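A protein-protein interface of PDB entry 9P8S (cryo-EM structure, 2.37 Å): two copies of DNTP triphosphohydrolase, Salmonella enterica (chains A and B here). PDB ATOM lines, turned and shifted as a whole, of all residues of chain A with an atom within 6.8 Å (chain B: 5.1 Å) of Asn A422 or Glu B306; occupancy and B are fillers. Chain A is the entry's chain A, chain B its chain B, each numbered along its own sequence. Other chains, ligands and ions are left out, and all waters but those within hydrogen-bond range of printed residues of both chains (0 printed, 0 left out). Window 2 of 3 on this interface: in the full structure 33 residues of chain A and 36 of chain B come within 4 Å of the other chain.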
ATOM      1  N   LYS A 172      -7.330  30.512 -29.042  1.00  0.00           N
ATOM      2  CA  LYS A 172      -6.594  29.679 -28.096  1.00  0.00           C
ATOM      3  C   LYS A 172      -5.113  30.024 -27.986  1.00  0.00           C
ATOM      4  O   LYS A 172      -4.399  29.369 -27.219  1.00  0.00           O
ATOM      5  CB  LYS A 172      -6.732  28.198 -28.468  1.00  0.00           C
ATOM      6  CG  LYS A 172      -8.115  27.792 -28.941  1.00  0.00           C
ATOM      7  CD  LYS A 172      -9.094  27.718 -27.787  1.00  0.00           C
ATOM      8  CE  LYS A 172      -8.995  26.386 -27.072  1.00  0.00           C
ATOM      9  NZ  LYS A 172      -9.295  25.254 -27.989  1.00  0.00           N
ATOM     10  N   LEU A 173      -4.625  31.025 -28.715  1.00  0.00           N
ATOM     11  CA  LEU A 173      -3.190  31.302 -28.789  1.00  0.00           C
ATOM     12  C   LEU A 173      -2.854  32.589 -28.042  1.00  0.00           C
ATOM     13  O   LEU A 173      -2.971  33.687 -28.592  1.00  0.00           O
ATOM     14  CB  LEU A 173      -2.723  31.379 -30.235  1.00  0.00           C
ATOM     15  CG  LEU A 173      -2.210  30.083 -30.863  1.00  0.00           C
ATOM     16  CD1 LEU A 173      -0.801  29.818 -30.371  1.00  0.00           C
ATOM     17  CD2 LEU A 173      -3.116  28.893 -30.585  1.00  0.00           C
ATOM     18  N   GLN A 174      -2.420  32.440 -26.793  1.00  0.00           N
ATOM     19  CA  GLN A 174      -1.846  33.539 -26.019  1.00  0.00           C
ATOM     20  C   GLN A 174      -1.212  33.016 -24.733  1.00  0.00           C
ATOM     21  O   GLN A 174      -1.843  33.007 -23.677  1.00  0.00           O
ATOM     22  CB  GLN A 174      -2.900  34.595 -25.686  1.00  0.00           C
ATOM     23  CG  GLN A 174      -2.339  36.005 -25.526  1.00  0.00           C
ATOM     24  CD  GLN A 174      -1.528  36.464 -26.728  1.00  0.00           C
ATOM     25  OE1 GLN A 174      -0.359  36.107 -26.884  1.00  0.00           O
ATOM     26  NE2 GLN A 174      -2.152  37.259 -27.588  1.00  0.00           N
ATOM     27  N   ILE A 419       9.829  23.466 -31.835  1.00  0.00           N
ATOM     28  CA  ILE A 419       8.454  23.925 -31.963  1.00  0.00           C
ATOM     29  C   ILE A 419       8.225  25.107 -31.028  1.00  0.00           C
ATOM     30  O   ILE A 419       8.814  25.196 -29.944  1.00  0.00           O
ATOM     31  CB  ILE A 419       7.478  22.772 -31.665  1.00  0.00           C
ATOM     32  CG1 ILE A 419       7.767  21.588 -32.584  1.00  0.00           C
ATOM     33  CG2 ILE A 419       6.036  23.214 -31.841  1.00  0.00           C
ATOM     34  CD1 ILE A 419       6.930  20.374 -32.285  1.00  0.00           C
ATOM     35  N   SER A 420       7.368  26.032 -31.459  1.00  0.00           N
ATOM     36  CA  SER A 420       7.076  27.212 -30.658  1.00  0.00           C
ATOM     37  C   SER A 420       6.494  26.812 -29.310  1.00  0.00           C
ATOM     38  O   SER A 420       5.754  25.831 -29.199  1.00  0.00           O
ATOM     39  CB  SER A 420       6.111  28.132 -31.404  1.00  0.00           C
ATOM     40  OG  SER A 420       5.504  29.053 -30.518  1.00  0.00           O
ATOM     41  N   GLU A 421       6.838  27.583 -28.276  1.00  0.00           N
ATOM     42  CA  GLU A 421       6.523  27.185 -26.910  1.00  0.00           C
ATOM     43  C   GLU A 421       5.024  27.170 -26.640  1.00  0.00           C
ATOM     44  O   GLU A 421       4.550  26.336 -25.862  1.00  0.00           O
ATOM     45  CB  GLU A 421       7.231  28.109 -25.920  1.00  0.00           C
ATOM     46  CG  GLU A 421       7.183  27.624 -24.482  1.00  0.00           C
ATOM     47  CD  GLU A 421       8.565  27.454 -23.882  1.00  0.00           C
ATOM     48  OE1 GLU A 421       9.558  27.588 -24.627  1.00  0.00           O
ATOM     49  OE2 GLU A 421       8.658  27.181 -22.667  1.00  0.00           O
ATOM     50  N   ASN A 422       4.264  28.084 -27.249  1.00  0.00           N
ATOM     51  CA  ASN A 422       2.826  28.119 -27.003  1.00  0.00           C
ATOM     52  C   ASN A 422       2.135  26.874 -27.548  1.00  0.00           C
ATOM     53  O   ASN A 422       1.225  26.333 -26.907  1.00  0.00           O
ATOM     54  CB  ASN A 422       2.220  29.383 -27.612  1.00  0.00           C
ATOM     55  CG  ASN A 422       2.723  29.653 -29.010  1.00  0.00           C
ATOM     56  OD1 ASN A 422       3.499  28.875 -29.562  1.00  0.00           O
ATOM     57  ND2 ASN A 422       2.292  30.766 -29.590  1.00  0.00           N
ATOM     58  N   TYR A 423       2.550  26.405 -28.727  1.00  0.00           N
ATOM     59  CA  TYR A 423       1.969  25.183 -29.276  1.00  0.00           C
ATOM     60  C   TYR A 423       2.243  23.991 -28.370  1.00  0.00           C
ATOM     61  O   TYR A 423       1.355  23.164 -28.135  1.00  0.00           O
ATOM     62  CB  TYR A 423       2.513  24.919 -30.679  1.00  0.00           C
ATOM     63  CG  TYR A 423       2.271  26.038 -31.662  1.00  0.00           C
ATOM     64  CD1 TYR A 423       1.062  26.714 -31.687  1.00  0.00           C
ATOM     65  CD2 TYR A 423       3.249  26.410 -32.570  1.00  0.00           C
ATOM     66  CE1 TYR A 423       0.836  27.731 -32.588  1.00  0.00           C
ATOM     67  CE2 TYR A 423       3.032  27.429 -33.474  1.00  0.00           C
ATOM     68  CZ  TYR A 423       1.824  28.087 -33.477  1.00  0.00           C
ATOM     69  OH  TYR A 423       1.600  29.102 -34.375  1.00  0.00           O
ATOM     70  N   ARG A 424       3.467  23.887 -27.853  1.00  0.00           N
ATOM     71  CA  ARG A 424       3.791  22.804 -26.931  1.00  0.00           C
ATOM     72  C   ARG A 424       2.994  22.925 -25.639  1.00  0.00           C
ATOM     73  O   ARG A 424       2.536  21.916 -25.089  1.00  0.00           O
ATOM     74  CB  ARG A 424       5.288  22.801 -26.638  1.00  0.00           C
ATOM     75  CG  ARG A 424       6.128  22.227 -27.757  1.00  0.00           C
ATOM     76  CD  ARG A 424       7.578  22.105 -27.339  1.00  0.00           C
ATOM     77  NE  ARG A 424       8.325  23.332 -27.583  1.00  0.00           N
ATOM     78  CZ  ARG A 424       9.043  23.964 -26.666  1.00  0.00           C
ATOM     79  NH1 ARG A 424       9.126  23.516 -25.424  1.00  0.00           N
ATOM     80  NH2 ARG A 424       9.697  25.071 -27.004  1.00  0.00           N
ATOM     81  N   ARG A 425       2.825  24.150 -25.137  1.00  0.00           N
ATOM     82  CA  ARG A 425       2.056  24.358 -23.917  1.00  0.00           C
ATOM     83  C   ARG A 425       0.613  23.912 -24.095  1.00  0.00           C
ATOM     84  O   ARG A 425       0.038  23.271 -23.207  1.00  0.00           O
ATOM     85  CB  ARG A 425       2.114  25.830 -23.516  1.00  0.00           C
ATOM     86  CG  ARG A 425       1.574  26.128 -22.132  1.00  0.00           C
ATOM     87  CD  ARG A 425       2.484  27.098 -21.395  1.00  0.00           C
ATOM     88  NE  ARG A 425       2.949  28.178 -22.258  1.00  0.00           N
ATOM     89  CZ  ARG A 425       2.180  29.148 -22.734  1.00  0.00           C
ATOM     90  NH1 ARG A 425       0.894  29.224 -22.431  1.00  0.00           N
ATOM     91  NH2 ARG A 425       2.715  30.068 -23.532  1.00  0.00           N
ATOM     92  N   ILE A 426       0.008  24.247 -25.236  1.00  0.00           N
ATOM     93  CA  ILE A 426      -1.341  23.766 -25.517  1.00  0.00           C
ATOM     94  C   ILE A 426      -1.348  22.252 -25.678  1.00  0.00           C
ATOM     95  O   ILE A 426      -2.302  21.582 -25.267  1.00  0.00           O
ATOM     96  CB  ILE A 426      -1.917  24.469 -26.759  1.00  0.00           C
ATOM     97  CG1 ILE A 426      -1.887  25.984 -26.571  1.00  0.00           C
ATOM     98  CG2 ILE A 426      -3.336  24.005 -27.027  1.00  0.00           C
ATOM     99  CD1 ILE A 426      -2.440  26.747 -27.744  1.00  0.00           C
ATOM    100  N   PHE A 427      -0.293  21.690 -26.270  1.00  0.00           N
ATOM    101  CA  PHE A 427      -0.216  20.242 -26.437  1.00  0.00           C
ATOM    102  C   PHE A 427      -0.147  19.522 -25.098  1.00  0.00           C
ATOM    103  O   PHE A 427      -0.727  18.443 -24.947  1.00  0.00           O
ATOM    104  CB  PHE A 427       0.989  19.879 -27.303  1.00  0.00           C
ATOM    105  CG  PHE A 427       1.260  18.405 -27.376  1.00  0.00           C
ATOM    106  CD1 PHE A 427       0.426  17.570 -28.096  1.00  0.00           C
ATOM    107  CD2 PHE A 427       2.356  17.857 -26.735  1.00  0.00           C
ATOM    108  CE1 PHE A 427       0.674  16.216 -28.166  1.00  0.00           C
ATOM    109  CE2 PHE A 427       2.608  16.504 -26.804  1.00  0.00           C
ATOM    110  CZ  PHE A 427       1.766  15.683 -27.520  1.00  0.00           C
ATOM    111  N   LEU A 442      -0.780  19.408 -32.763  1.00  0.00           N
ATOM    112  CA  LEU A 442       0.503  20.054 -32.507  1.00  0.00           C
ATOM    113  C   LEU A 442       1.293  20.207 -33.798  1.00  0.00           C
ATOM    114  O   LEU A 442       1.853  21.276 -34.077  1.00  0.00           O
ATOM    115  CB  LEU A 442       1.299  19.253 -31.478  1.00  0.00           C
ATOM    116  CG  LEU A 442       2.760  19.661 -31.285  1.00  0.00           C
ATOM    117  CD1 LEU A 442       2.866  21.121 -30.882  1.00  0.00           C
ATOM    118  CD2 LEU A 442       3.430  18.773 -30.254  1.00  0.00           C
ATOM    119  N   LEU B 302       5.074  30.657 -17.774  1.00  0.00           N
ATOM    120  CA  LEU B 302       5.459  31.018 -19.128  1.00  0.00           C
ATOM    121  C   LEU B 302       6.973  31.154 -19.216  1.00  0.00           C
ATOM    122  O   LEU B 302       7.646  31.445 -18.223  1.00  0.00           O
ATOM    123  CB  LEU B 302       4.801  32.330 -19.569  1.00  0.00           C
ATOM    124  CG  LEU B 302       3.305  32.494 -19.298  1.00  0.00           C
ATOM    125  CD1 LEU B 302       2.878  33.933 -19.531  1.00  0.00           C
ATOM    126  CD2 LEU B 302       2.498  31.548 -20.168  1.00  0.00           C
ATOM    127  N   SER B 303       7.498  30.936 -20.418  1.00  0.00           N
ATOM    128  CA  SER B 303       8.911  31.163 -20.660  1.00  0.00           C
ATOM    129  C   SER B 303       9.227  32.649 -20.488  1.00  0.00           C
ATOM    130  O   SER B 303       8.348  33.499 -20.660  1.00  0.00           O
ATOM    131  CB  SER B 303       9.289  30.697 -22.065  1.00  0.00           C
ATOM    132  OG  SER B 303      10.332  31.485 -22.610  1.00  0.00           O
ATOM    133  N   PRO B 304      10.468  32.991 -20.126  1.00  0.00           N
ATOM    134  CA  PRO B 304      10.810  34.414 -19.962  1.00  0.00           C
ATOM    135  C   PRO B 304      10.507  35.250 -21.192  1.00  0.00           C
ATOM    136  O   PRO B 304      10.046  36.392 -21.065  1.00  0.00           O
ATOM    137  CB  PRO B 304      12.313  34.375 -19.656  1.00  0.00           C
ATOM    138  CG  PRO B 304      12.538  33.034 -19.055  1.00  0.00           C
ATOM    139  CD  PRO B 304      11.580  32.105 -19.741  1.00  0.00           C
ATOM    140  N   ALA B 305      10.739  34.703 -22.388  1.00  0.00           N
ATOM    141  CA  ALA B 305      10.370  35.413 -23.607  1.00  0.00           C
ATOM    142  C   ALA B 305       8.863  35.622 -23.687  1.00  0.00           C
ATOM    143  O   ALA B 305       8.401  36.703 -24.064  1.00  0.00           O
ATOM    144  CB  ALA B 305      10.875  34.651 -24.831  1.00  0.00           C
ATOM    145  N   GLU B 306       8.081  34.599 -23.335  1.00  0.00           N
ATOM    146  CA  GLU B 306       6.627  34.723 -23.385  1.00  0.00           C
ATOM    147  C   GLU B 306       6.116  35.744 -22.376  1.00  0.00           C
ATOM    148  O   GLU B 306       5.228  36.548 -22.690  1.00  0.00           O
ATOM    149  CB  GLU B 306       5.982  33.360 -23.142  1.00  0.00           C
ATOM    150  CG  GLU B 306       6.345  32.316 -24.184  1.00  0.00           C
ATOM    151  CD  GLU B 306       5.654  30.991 -23.945  1.00  0.00           C
ATOM    152  OE1 GLU B 306       5.915  30.365 -22.896  1.00  0.00           O
ATOM    153  OE2 GLU B 306       4.848  30.575 -24.802  1.00  0.00           O
ATOM    154  N   LEU B 307       6.654  35.719 -21.155  1.00  0.00           N
ATOM    155  CA  LEU B 307       6.253  36.698 -20.151  1.00  0.00           C
ATOM    156  C   LEU B 307       6.621  38.109 -20.587  1.00  0.00           C
ATOM    157  O   LEU B 307       5.828  39.046 -20.427  1.00  0.00           O
ATOM    158  CB  LEU B 307       6.899  36.367 -18.807  1.00  0.00           C
ATOM    159  CG  LEU B 307       6.462  37.228 -17.622  1.00  0.00           C
ATOM    160  CD1 LEU B 307       4.963  37.113 -17.407  1.00  0.00           C
ATOM    161  CD2 LEU B 307       7.220  36.833 -16.368  1.00  0.00           C
ATOM    162  N   ASN B 308       7.823  38.276 -21.145  1.00  0.00           N
ATOM    163  CA  ASN B 308       8.223  39.581 -21.656  1.00  0.00           C
ATOM    164  C   ASN B 308       7.291  40.042 -22.765  1.00  0.00           C
ATOM    165  O   ASN B 308       6.898  41.212 -22.807  1.00  0.00           O
ATOM    166  CB  ASN B 308       9.665  39.528 -22.159  1.00  0.00           C
ATOM    167  CG  ASN B 308      10.664  39.954 -21.108  1.00  0.00           C
ATOM    168  OD1 ASN B 308      10.564  41.044 -20.547  1.00  0.00           O
ATOM    169  ND2 ASN B 308      11.637  39.095 -20.836  1.00  0.00           N
ATOM    170  N   ASP B 309       6.919  39.134 -23.670  1.00  0.00           N
ATOM    171  CA  ASP B 309       6.029  39.497 -24.767  1.00  0.00           C
ATOM    172  C   ASP B 309       4.663  39.930 -24.255  1.00  0.00           C
ATOM    173  O   ASP B 309       4.113  40.936 -24.713  1.00  0.00           O
ATOM    174  CB  ASP B 309       5.888  38.327 -25.737  1.00  0.00           C
ATOM    175  CG  ASP B 309       7.139  38.096 -26.557  1.00  0.00           C
ATOM    176  OD1 ASP B 309       7.210  37.066 -27.260  1.00  0.00           O
ATOM    177  OD2 ASP B 309       8.053  38.945 -26.499  1.00  0.00           O
ATOM    178  N   MET B 310       4.097  39.183 -23.304  1.00  0.00           N
ATOM    179  CA  MET B 310       2.781  39.535 -22.779  1.00  0.00           C
ATOM    180  C   MET B 310       2.820  40.872 -22.046  1.00  0.00           C
ATOM    181  O   MET B 310       1.945  41.731 -22.237  1.00  0.00           O
ATOM    182  CB  MET B 310       2.273  38.427 -21.858  1.00  0.00           C
ATOM    183  CG  MET B 310       1.883  37.155 -22.584  1.00  0.00           C
ATOM    184  SD  MET B 310       0.121  37.082 -22.946  1.00  0.00           S
ATOM    185  CE  MET B 310      -0.517  36.492 -21.380  1.00  0.00           C
ATOM    186  N   SER B 311       3.838  41.068 -21.204  1.00  0.00           N
ATOM    187  CA  SER B 311       3.956  42.325 -20.476  1.00  0.00           C
ATOM    188  C   SER B 311       4.154  43.494 -21.428  1.00  0.00           C
ATOM    189  O   SER B 311       3.564  44.563 -21.241  1.00  0.00           O
ATOM    190  CB  SER B 311       5.105  42.243 -19.474  1.00  0.00           C
ATOM    191  OG  SER B 311       4.942  41.137 -18.606  1.00  0.00           O
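The guanidinium group (NH2) of Arg A425 is in salt-bridge range of the side-chain carboxylate (OE2) of Glu B306 (2.5 Å).
The guanidinium group (NH2) of Arg A424 is in salt-bridge range of the side-chain carboxylate (OE1) of Glu A421 (3.5 Å). OG of Ser B303 sits close to N of Ala B305. The backbone NH (N) of Ser B303 sits at hydrogen-bond distance from the side-chain carboxylate (OE1) of Glu B306 (3.0 Å).
Among the printed residues, merely in contact across the chains: Glu A421 with Glu B306 (3.4 Å), Arg A425 with Leu B302 (3.5 Å), Asn A422 with Glu B306 (3.5 Å), Glu A421 with Ser B303 (3.6 Å) and Gln A174 with Met B310 (3.7 Å).
Of chain B, only Glu B306 comes within 4 Å of Asn A422. Of the printed residues of chain A, Met B310 touches Gln A174. Of the printed residues of chain A, Leu B302 touches Arg A425 (3.5 Å). Printed residues of chain B within 4 Å of Glu A421: Ser B303 and Glu B306. Printed residues of chain B within 4 Å of Gln A174: Met B310. Ser B311 touches none of the printed residues of chain A. Leu B307 touches none of the printed residues of chain A. The nearest residue of chain A that does not touch Glu B306 is Ser A420 (6.0 Å).
Of the 13 printed residues of chain A, 4 touch a printed residue of chain B. Of the 10 printed residues of chain B, 4 touch a printed residue of chain A. Hydrophobic or aromatic side chains of chain B that line the printed part of chain A: Leu B302 and Met B310.
No position is printed for both chains.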
